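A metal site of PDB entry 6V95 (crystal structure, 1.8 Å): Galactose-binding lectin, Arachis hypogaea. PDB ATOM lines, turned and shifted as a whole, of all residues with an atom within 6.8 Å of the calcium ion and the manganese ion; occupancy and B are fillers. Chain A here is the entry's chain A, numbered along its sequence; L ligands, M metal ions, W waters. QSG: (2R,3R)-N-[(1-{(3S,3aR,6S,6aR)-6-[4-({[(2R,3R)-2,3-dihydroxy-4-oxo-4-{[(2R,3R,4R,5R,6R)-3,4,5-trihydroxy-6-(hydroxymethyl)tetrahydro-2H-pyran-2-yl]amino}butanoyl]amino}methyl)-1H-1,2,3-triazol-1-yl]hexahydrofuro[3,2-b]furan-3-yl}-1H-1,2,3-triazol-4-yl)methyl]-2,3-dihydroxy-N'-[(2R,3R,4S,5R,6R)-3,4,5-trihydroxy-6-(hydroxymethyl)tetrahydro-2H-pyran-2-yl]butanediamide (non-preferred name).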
ATOM      1  N   ASP A  83      -5.596   1.118  33.582  1.00  0.00           N
ATOM      2  CA  ASP A  83      -5.005   0.898  32.251  1.00  0.00           C
ATOM      3  C   ASP A  83      -3.606   0.308  32.264  1.00  0.00           C
ATOM      4  O   ASP A  83      -3.139  -0.129  31.218  1.00  0.00           O
ATOM      5  CB  ASP A  83      -4.979   2.200  31.476  1.00  0.00           C
ATOM      6  CG  ASP A  83      -6.294   2.441  30.789  1.00  0.00           C
ATOM      7  OD1 ASP A  83      -7.195   3.066  31.425  1.00  0.00           O
ATOM      8  OD2 ASP A  83      -6.478   1.913  29.675  1.00  0.00           O
ATOM      9  N   GLY A 103      -6.388   7.153  31.179  1.00  0.00           N
ATOM     10  CA  GLY A 103      -6.662   6.027  30.287  1.00  0.00           C
ATOM     11  C   GLY A 103      -5.404   5.437  29.634  1.00  0.00           C
ATOM     12  O   GLY A 103      -4.438   5.111  30.333  1.00  0.00           O
ATOM     13  N   GLY A 104      -5.455   5.331  28.305  1.00  0.00           N
ATOM     14  CA  GLY A 104      -4.391   4.759  27.485  1.00  0.00           C
ATOM     15  C   GLY A 104      -3.095   5.551  27.434  1.00  0.00           C
ATOM     16  O   GLY A 104      -2.067   5.033  26.986  1.00  0.00           O
ATOM     17  N   THR A 105      -3.163   6.826  27.843  1.00  0.00           N
ATOM     18  CA  THR A 105      -2.002   7.716  27.879  1.00  0.00           C
ATOM     19  C   THR A 105      -0.995   7.292  28.984  1.00  0.00           C
ATOM     20  O   THR A 105       0.113   7.797  28.995  1.00  0.00           O
ATOM     21  CB  THR A 105      -2.444   9.191  28.090  1.00  0.00           C
ATOM     22  OG1 THR A 105      -2.817   9.408  29.452  1.00  0.00           O
ATOM     23  CG2 THR A 105      -3.544   9.623  27.118  1.00  0.00           C
ATOM     24  N   LEU A 106      -1.439   6.459  29.972  1.00  0.00           N
ATOM     25  CA  LEU A 106      -0.666   5.946  31.118  1.00  0.00           C
ATOM     26  C   LEU A 106      -0.044   7.091  31.979  1.00  0.00           C
ATOM     27  O   LEU A 106       0.899   6.856  32.754  1.00  0.00           O
ATOM     28  CB  LEU A 106       0.426   4.941  30.658  1.00  0.00           C
ATOM     29  CG  LEU A 106      -0.054   3.709  29.897  1.00  0.00           C
ATOM     30  CD1 LEU A 106       1.136   2.837  29.481  1.00  0.00           C
ATOM     31  CD2 LEU A 106      -1.072   2.871  30.718  1.00  0.00           C
ATOM     32  N   GLU A 121       6.227  -0.078  29.639  1.00  0.00           N
ATOM     33  CA  GLU A 121       4.840  -0.154  30.051  1.00  0.00           C
ATOM     34  C   GLU A 121       4.379  -1.602  30.281  1.00  0.00           C
ATOM     35  O   GLU A 121       4.797  -2.528  29.574  1.00  0.00           O
ATOM     36  CB  GLU A 121       3.933   0.524  29.011  1.00  0.00           C
ATOM     37  CG  GLU A 121       4.103  -0.100  27.629  1.00  0.00           C
ATOM     38  CD  GLU A 121       2.982   0.304  26.721  1.00  0.00           C
ATOM     39  OE1 GLU A 121       2.825   1.526  26.510  1.00  0.00           O
ATOM     40  OE2 GLU A 121       2.202  -0.577  26.296  1.00  0.00           O
ATOM     41  N   ASP A 123       0.943  -2.800  30.154  1.00  0.00           N
ATOM     42  CA  ASP A 123      -0.340  -2.354  29.634  1.00  0.00           C
ATOM     43  C   ASP A 123      -1.425  -3.425  29.690  1.00  0.00           C
ATOM     44  O   ASP A 123      -1.245  -4.514  29.144  1.00  0.00           O
ATOM     45  CB  ASP A 123      -0.112  -1.884  28.200  1.00  0.00           C
ATOM     46  CG  ASP A 123      -1.224  -1.048  27.628  1.00  0.00           C
ATOM     47  OD1 ASP A 123      -2.321  -0.979  28.246  1.00  0.00           O
ATOM     48  OD2 ASP A 123      -1.010  -0.439  26.565  1.00  0.00           O
ATOM     49  N   THR A 124      -2.567  -3.111  30.376  1.00  0.00           N
ATOM     50  CA  THR A 124      -3.642  -4.084  30.602  1.00  0.00           C
ATOM     51  C   THR A 124      -4.945  -3.776  29.837  1.00  0.00           C
ATOM     52  O   THR A 124      -5.971  -4.420  30.110  1.00  0.00           O
ATOM     53  CB  THR A 124      -3.910  -4.208  32.107  1.00  0.00           C
ATOM     54  OG1 THR A 124      -4.637  -3.067  32.563  1.00  0.00           O
ATOM     55  CG2 THR A 124      -2.638  -4.364  32.930  1.00  0.00           C
ATOM     56  N   TYR A 125      -4.913  -2.862  28.851  1.00  0.00           N
ATOM     57  CA  TYR A 125      -6.094  -2.502  28.041  1.00  0.00           C
ATOM     58  C   TYR A 125      -5.655  -2.136  26.625  1.00  0.00           C
ATOM     59  O   TYR A 125      -4.747  -1.309  26.462  1.00  0.00           O
ATOM     60  CB  TYR A 125      -6.911  -1.360  28.661  1.00  0.00           C
ATOM     61  CG  TYR A 125      -8.187  -1.107  27.876  1.00  0.00           C
ATOM     62  CD1 TYR A 125      -9.350  -1.822  28.159  1.00  0.00           C
ATOM     63  CD2 TYR A 125      -8.209  -0.219  26.804  1.00  0.00           C
ATOM     64  CE1 TYR A 125     -10.514  -1.605  27.421  1.00  0.00           C
ATOM     65  CE2 TYR A 125      -9.342  -0.056  26.024  1.00  0.00           C
ATOM     66  CZ  TYR A 125     -10.492  -0.753  26.332  1.00  0.00           C
ATOM     67  OH  TYR A 125     -11.644  -0.564  25.595  1.00  0.00           O
ATOM     68  N   SER A 126      -6.303  -2.731  25.607  1.00  0.00           N
ATOM     69  CA  SER A 126      -5.945  -2.520  24.199  1.00  0.00           C
ATOM     70  C   SER A 126      -6.596  -1.254  23.630  1.00  0.00           C
ATOM     71  O   SER A 126      -7.803  -1.233  23.391  1.00  0.00           O
ATOM     72  CB  SER A 126      -6.311  -3.738  23.359  1.00  0.00           C
ATOM     73  OG  SER A 126      -5.856  -3.613  22.022  1.00  0.00           O
ATOM     74  N   ASN A 127      -5.785  -0.197  23.467  1.00  0.00           N
ATOM     75  CA  ASN A 127      -6.180   1.093  22.903  1.00  0.00           C
ATOM     76  C   ASN A 127      -5.877   1.113  21.406  1.00  0.00           C
ATOM     77  O   ASN A 127      -4.732   1.347  21.018  1.00  0.00           O
ATOM     78  CB  ASN A 127      -5.480   2.245  23.612  1.00  0.00           C
ATOM     79  CG  ASN A 127      -5.841   2.373  25.059  1.00  0.00           C
ATOM     80  OD1 ASN A 127      -5.387   1.611  25.919  1.00  0.00           O
ATOM     81  ND2 ASN A 127      -6.640   3.380  25.380  1.00  0.00           N
ATOM     82  N   TYR A 130      -3.848   3.916  19.884  1.00  0.00           N
ATOM     83  CA  TYR A 130      -2.389   3.894  20.091  1.00  0.00           C
ATOM     84  C   TYR A 130      -1.741   2.625  19.489  1.00  0.00           C
ATOM     85  O   TYR A 130      -0.602   2.294  19.810  1.00  0.00           O
ATOM     86  CB  TYR A 130      -2.043   4.015  21.584  1.00  0.00           C
ATOM     87  CG  TYR A 130      -2.684   5.214  22.248  1.00  0.00           C
ATOM     88  CD1 TYR A 130      -2.657   6.468  21.640  1.00  0.00           C
ATOM     89  CD2 TYR A 130      -3.307   5.110  23.495  1.00  0.00           C
ATOM     90  CE1 TYR A 130      -3.260   7.571  22.235  1.00  0.00           C
ATOM     91  CE2 TYR A 130      -3.933   6.202  24.077  1.00  0.00           C
ATOM     92  CZ  TYR A 130      -3.900   7.426  23.451  1.00  0.00           C
ATOM     93  OH  TYR A 130      -4.486   8.514  24.044  1.00  0.00           O
ATOM     94  N   ASN A 131      -2.485   1.949  18.586  1.00  0.00           N
ATOM     95  CA  ASN A 131      -2.086   0.720  17.882  1.00  0.00           C
ATOM     96  C   ASN A 131      -1.617  -0.380  18.868  1.00  0.00           C
ATOM     97  O   ASN A 131      -0.670  -1.113  18.574  1.00  0.00           O
ATOM     98  CB  ASN A 131      -1.016   1.026  16.808  1.00  0.00           C
ATOM     99  CG  ASN A 131      -1.541   1.888  15.678  1.00  0.00           C
ATOM    100  OD1 ASN A 131      -2.538   1.558  15.014  1.00  0.00           O
ATOM    101  ND2 ASN A 131      -0.888   3.015  15.444  1.00  0.00           N
ATOM    102  N   ASP A 132      -2.309  -0.484  20.018  1.00  0.00           N
ATOM    103  CA  ASP A 132      -1.999  -1.511  21.028  1.00  0.00           C
ATOM    104  C   ASP A 132      -2.195  -2.917  20.466  1.00  0.00           C
ATOM    105  O   ASP A 132      -3.162  -3.117  19.718  1.00  0.00           O
ATOM    106  CB  ASP A 132      -2.894  -1.362  22.260  1.00  0.00           C
ATOM    107  CG  ASP A 132      -2.336  -0.519  23.380  1.00  0.00           C
ATOM    108  OD1 ASP A 132      -1.105  -0.351  23.432  1.00  0.00           O
ATOM    109  OD2 ASP A 132      -3.121  -0.064  24.232  1.00  0.00           O
ATOM    110  N   PRO A 133      -1.404  -3.921  20.876  1.00  0.00           N
ATOM    111  CA  PRO A 133      -1.683  -5.294  20.407  1.00  0.00           C
ATOM    112  C   PRO A 133      -3.000  -5.789  21.057  1.00  0.00           C
ATOM    113  O   PRO A 133      -3.465  -5.148  21.996  1.00  0.00           O
ATOM    114  CB  PRO A 133      -0.446  -6.092  20.830  1.00  0.00           C
ATOM    115  CG  PRO A 133       0.167  -5.313  21.934  1.00  0.00           C
ATOM    116  CD  PRO A 133      -0.199  -3.875  21.748  1.00  0.00           C
ATOM    117  N   HIS A 137       0.251  -6.614  27.428  1.00  0.00           N
ATOM    118  CA  HIS A 137       1.603  -6.602  26.879  1.00  0.00           C
ATOM    119  C   HIS A 137       2.571  -5.723  27.660  1.00  0.00           C
ATOM    120  O   HIS A 137       2.162  -4.794  28.365  1.00  0.00           O
ATOM    121  CB  HIS A 137       1.549  -6.104  25.396  1.00  0.00           C
ATOM    122  CG  HIS A 137       0.865  -4.782  25.240  1.00  0.00           C
ATOM    123  ND1 HIS A 137      -0.540  -4.662  25.264  1.00  0.00           N
ATOM    124  CD2 HIS A 137       1.397  -3.552  25.077  1.00  0.00           C
ATOM    125  CE1 HIS A 137      -0.783  -3.377  25.111  1.00  0.00           C
ATOM    126  NE2 HIS A 137       0.350  -2.669  24.985  1.00  0.00           N
ATOM    127  N   VAL A 138       3.852  -6.044  27.505  1.00  0.00           N
ATOM    128  CA  VAL A 138       4.961  -5.236  27.993  1.00  0.00           C
ATOM    129  C   VAL A 138       5.459  -4.520  26.766  1.00  0.00           C
ATOM    130  O   VAL A 138       5.632  -5.140  25.710  1.00  0.00           O
ATOM    131  CB  VAL A 138       6.065  -6.035  28.741  1.00  0.00           C
ATOM    132  CG1 VAL A 138       7.179  -5.105  29.228  1.00  0.00           C
ATOM    133  CG2 VAL A 138       5.488  -6.831  29.910  1.00  0.00           C
ATOM    134  N   GLY A 139       5.596  -3.212  26.865  1.00  0.00           N
ATOM    135  CA  GLY A 139       6.063  -2.418  25.739  1.00  0.00           C
ATOM    136  C   GLY A 139       7.245  -1.541  26.068  1.00  0.00           C
ATOM    137  O   GLY A 139       7.451  -1.166  27.222  1.00  0.00           O
ATOM    138  N   ASP A 141       8.666   2.066  25.097  1.00  0.00           N
ATOM    139  CA  ASP A 141       8.118   3.326  24.615  1.00  0.00           C
ATOM    140  C   ASP A 141       9.166   4.411  24.504  1.00  0.00           C
ATOM    141  O   ASP A 141       9.958   4.628  25.417  1.00  0.00           O
ATOM    142  CB  ASP A 141       7.006   3.805  25.571  1.00  0.00           C
ATOM    143  CG  ASP A 141       5.769   2.930  25.628  1.00  0.00           C
ATOM    144  OD1 ASP A 141       5.685   1.977  24.830  1.00  0.00           O
ATOM    145  OD2 ASP A 141       4.904   3.196  26.482  1.00  0.00           O
ATOM    146  N   VAL A 145       3.084   6.349  23.514  1.00  0.00           N
ATOM    147  CA  VAL A 145       2.445   5.152  24.051  1.00  0.00           C
ATOM    148  C   VAL A 145       2.081   4.205  22.870  1.00  0.00           C
ATOM    149  O   VAL A 145       1.542   3.116  23.084  1.00  0.00           O
ATOM    150  CB  VAL A 145       1.253   5.401  25.026  1.00  0.00           C
ATOM    151  CG1 VAL A 145       1.734   6.043  26.329  1.00  0.00           C
ATOM    152  CG2 VAL A 145       0.147   6.215  24.382  1.00  0.00           C
ATOM    153  N   ASP A 146       2.436   4.606  21.610  1.00  0.00           N
ATOM    154  CA  ASP A 146       2.400   3.706  20.473  1.00  0.00           C
ATOM    155  C   ASP A 146       3.794   3.081  20.494  1.00  0.00           C
ATOM    156  O   ASP A 146       4.756   3.655  19.966  1.00  0.00           O
ATOM    157  CB  ASP A 146       2.062   4.446  19.150  1.00  0.00           C
ATOM    158  CG  ASP A 146       1.887   3.547  17.916  1.00  0.00           C
ATOM    159  OD1 ASP A 146       2.382   2.388  17.932  1.00  0.00           O
ATOM    160  OD2 ASP A 146       1.286   3.999  16.919  1.00  0.00           O
ATOM    161  N   SER A 147       3.928   1.990  21.260  1.00  0.00           N
ATOM    162  CA  SER A 147       5.215   1.350  21.536  1.00  0.00           C
ATOM    163  C   SER A 147       6.082   1.069  20.293  1.00  0.00           C
ATOM    164  O   SER A 147       5.587   0.659  19.219  1.00  0.00           O
ATOM    165  CB  SER A 147       5.026   0.042  22.297  1.00  0.00           C
ATOM    166  OG  SER A 147       4.291   0.172  23.506  1.00  0.00           O
ATOM    167  N   THR A 150       6.498  -4.370  21.450  1.00  0.00           N
ATOM    168  CA  THR A 150       5.736  -5.011  22.510  1.00  0.00           C
ATOM    169  C   THR A 150       5.997  -6.503  22.504  1.00  0.00           C
ATOM    170  O   THR A 150       6.458  -7.061  21.490  1.00  0.00           O
ATOM    171  CB  THR A 150       4.202  -4.745  22.412  1.00  0.00           C
ATOM    172  OG1 THR A 150       3.650  -5.434  21.296  1.00  0.00           O
ATOM    173  CG2 THR A 150       3.832  -3.280  22.402  1.00  0.00           C
HETATM  174  N1  QSG L   1     -12.555   4.799  27.194  1.00  0.00           N
HETATM  175  C4  QSG L   1      -9.698   2.241  29.018  1.00  0.00           C
HETATM  176  C3  QSG L   1      -9.222   3.214  27.933  1.00  0.00           C
HETATM  177  C5  QSG L   1     -11.155   1.846  28.743  1.00  0.00           C
HETATM  178  C1  QSG L   1     -11.577   3.783  27.413  1.00  0.00           C
HETATM  179  C2  QSG L   1     -10.175   4.359  27.621  1.00  0.00           C
HETATM  180  C6  QSG L   1     -11.798   1.029  29.830  1.00  0.00           C
HETATM  181  C7  QSG L   1     -13.642   4.580  26.443  1.00  0.00           C
HETATM  182  C8  QSG L   1     -14.562   5.761  26.136  1.00  0.00           C
HETATM  183  C9  QSG L   1     -16.002   5.388  26.528  1.00  0.00           C
HETATM  184  C10 QSG L   1     -16.988   6.146  25.647  1.00  0.00           C
HETATM  185  O5  QSG L   1     -11.953   3.019  28.571  1.00  0.00           O
HETATM  186  O2  QSG L   1      -9.759   5.041  26.445  1.00  0.00           O
HETATM  187  O3  QSG L   1      -7.863   3.627  28.054  1.00  0.00           O
HETATM  188  O4  QSG L   1      -9.636   2.799  30.332  1.00  0.00           O
HETATM  189  O6  QSG L   1     -12.962   0.339  29.359  1.00  0.00           O
HETATM  190  O10 QSG L   1     -16.852   6.148  24.424  1.00  0.00           O
HETATM  191  O9  QSG L   1     -16.246   5.619  27.913  1.00  0.00           O
HETATM  192  O8  QSG L   1     -14.137   6.943  26.784  1.00  0.00           O
HETATM  193  O7  QSG L   1     -13.926   3.478  25.993  1.00  0.00           O
HETATM  194 CA    CA M   1      -3.361   0.379  26.531  1.00  0.00          CA
HETATM  195 MN    MN M   2       0.391  -0.612  24.935  1.00  0.00          MN
HETATM  196  O   HOH W   1       1.694  -0.751  23.296  1.00  0.00           O
HETATM  197  O   HOH W   2       0.517   1.744  25.148  1.00  0.00           O
HETATM  198  O   HOH W   3      -2.023   2.459  26.263  1.00  0.00           O
HETATM  199  O   HOH W   4      -3.970   1.143  28.599  1.00  0.00           O
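N of Gly 104 sits at hydrogen-bond distance from O3 of the ligand, at 3.0 Å. OD1 of Asp 83 sits at hydrogen-bond distance from O4 of the ligand, 2.7 Å away. O3 of the ligand is in hydrogen-bond range of ND2 of Asn 127 (3.0 Å).
The side-chain carboxylate (OD2) of Asp 141 lies close to the side-chain carboxylate (OE1) of Glu 121. The backbone carbonyl oxygen of Glu 121 is in hydrogen-bond range of the backbone NH of Gly 139 (2.9 Å).
Within 4 Å of the manganese ion: Glu 121, Asp 123, Asp 132 and His 137. The nearest printed residue that does not touch the manganese ion is Ser 147 (4.2 Å).
The calcium ion is bound by O of Tyr 125 (2.2 Å). Water W4 binds the calcium ion (2.3 Å). The side-chain carboxylate (OD2) of Asp 132 binds the calcium ion, 2.4 Å away. The calcium ion is bound by OD1 of Asp 123, at 2.4 Å. OD1 of Asn 127 is bound to the calcium ion. Water W3 is bound to the calcium ion (2.5 Å). OD2 of Asp 123 is bound to the calcium ion, at 2.5 Å. The calcium ion has seven donor atoms within binding distance.
NE2 of His 137 binds the manganese ion (2.1 Å). Water W1 binds the manganese ion. The side-chain carboxylate (OD1) of Asp 132 is bound to the manganese ion (2.1 Å). The side-chain carboxylate (OD2) of Asp 123 binds the manganese ion (2.2 Å). OE2 of Glu 121 is bound to the manganese ion (2.3 Å). The manganese ion is bound by water W2, 2.4 Å away. The manganese ion has six donor atoms within binding distance.
Water W2 bridges the backbone carbonyl oxygen of Val 145 and the side-chain carboxylate of Glu 121.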
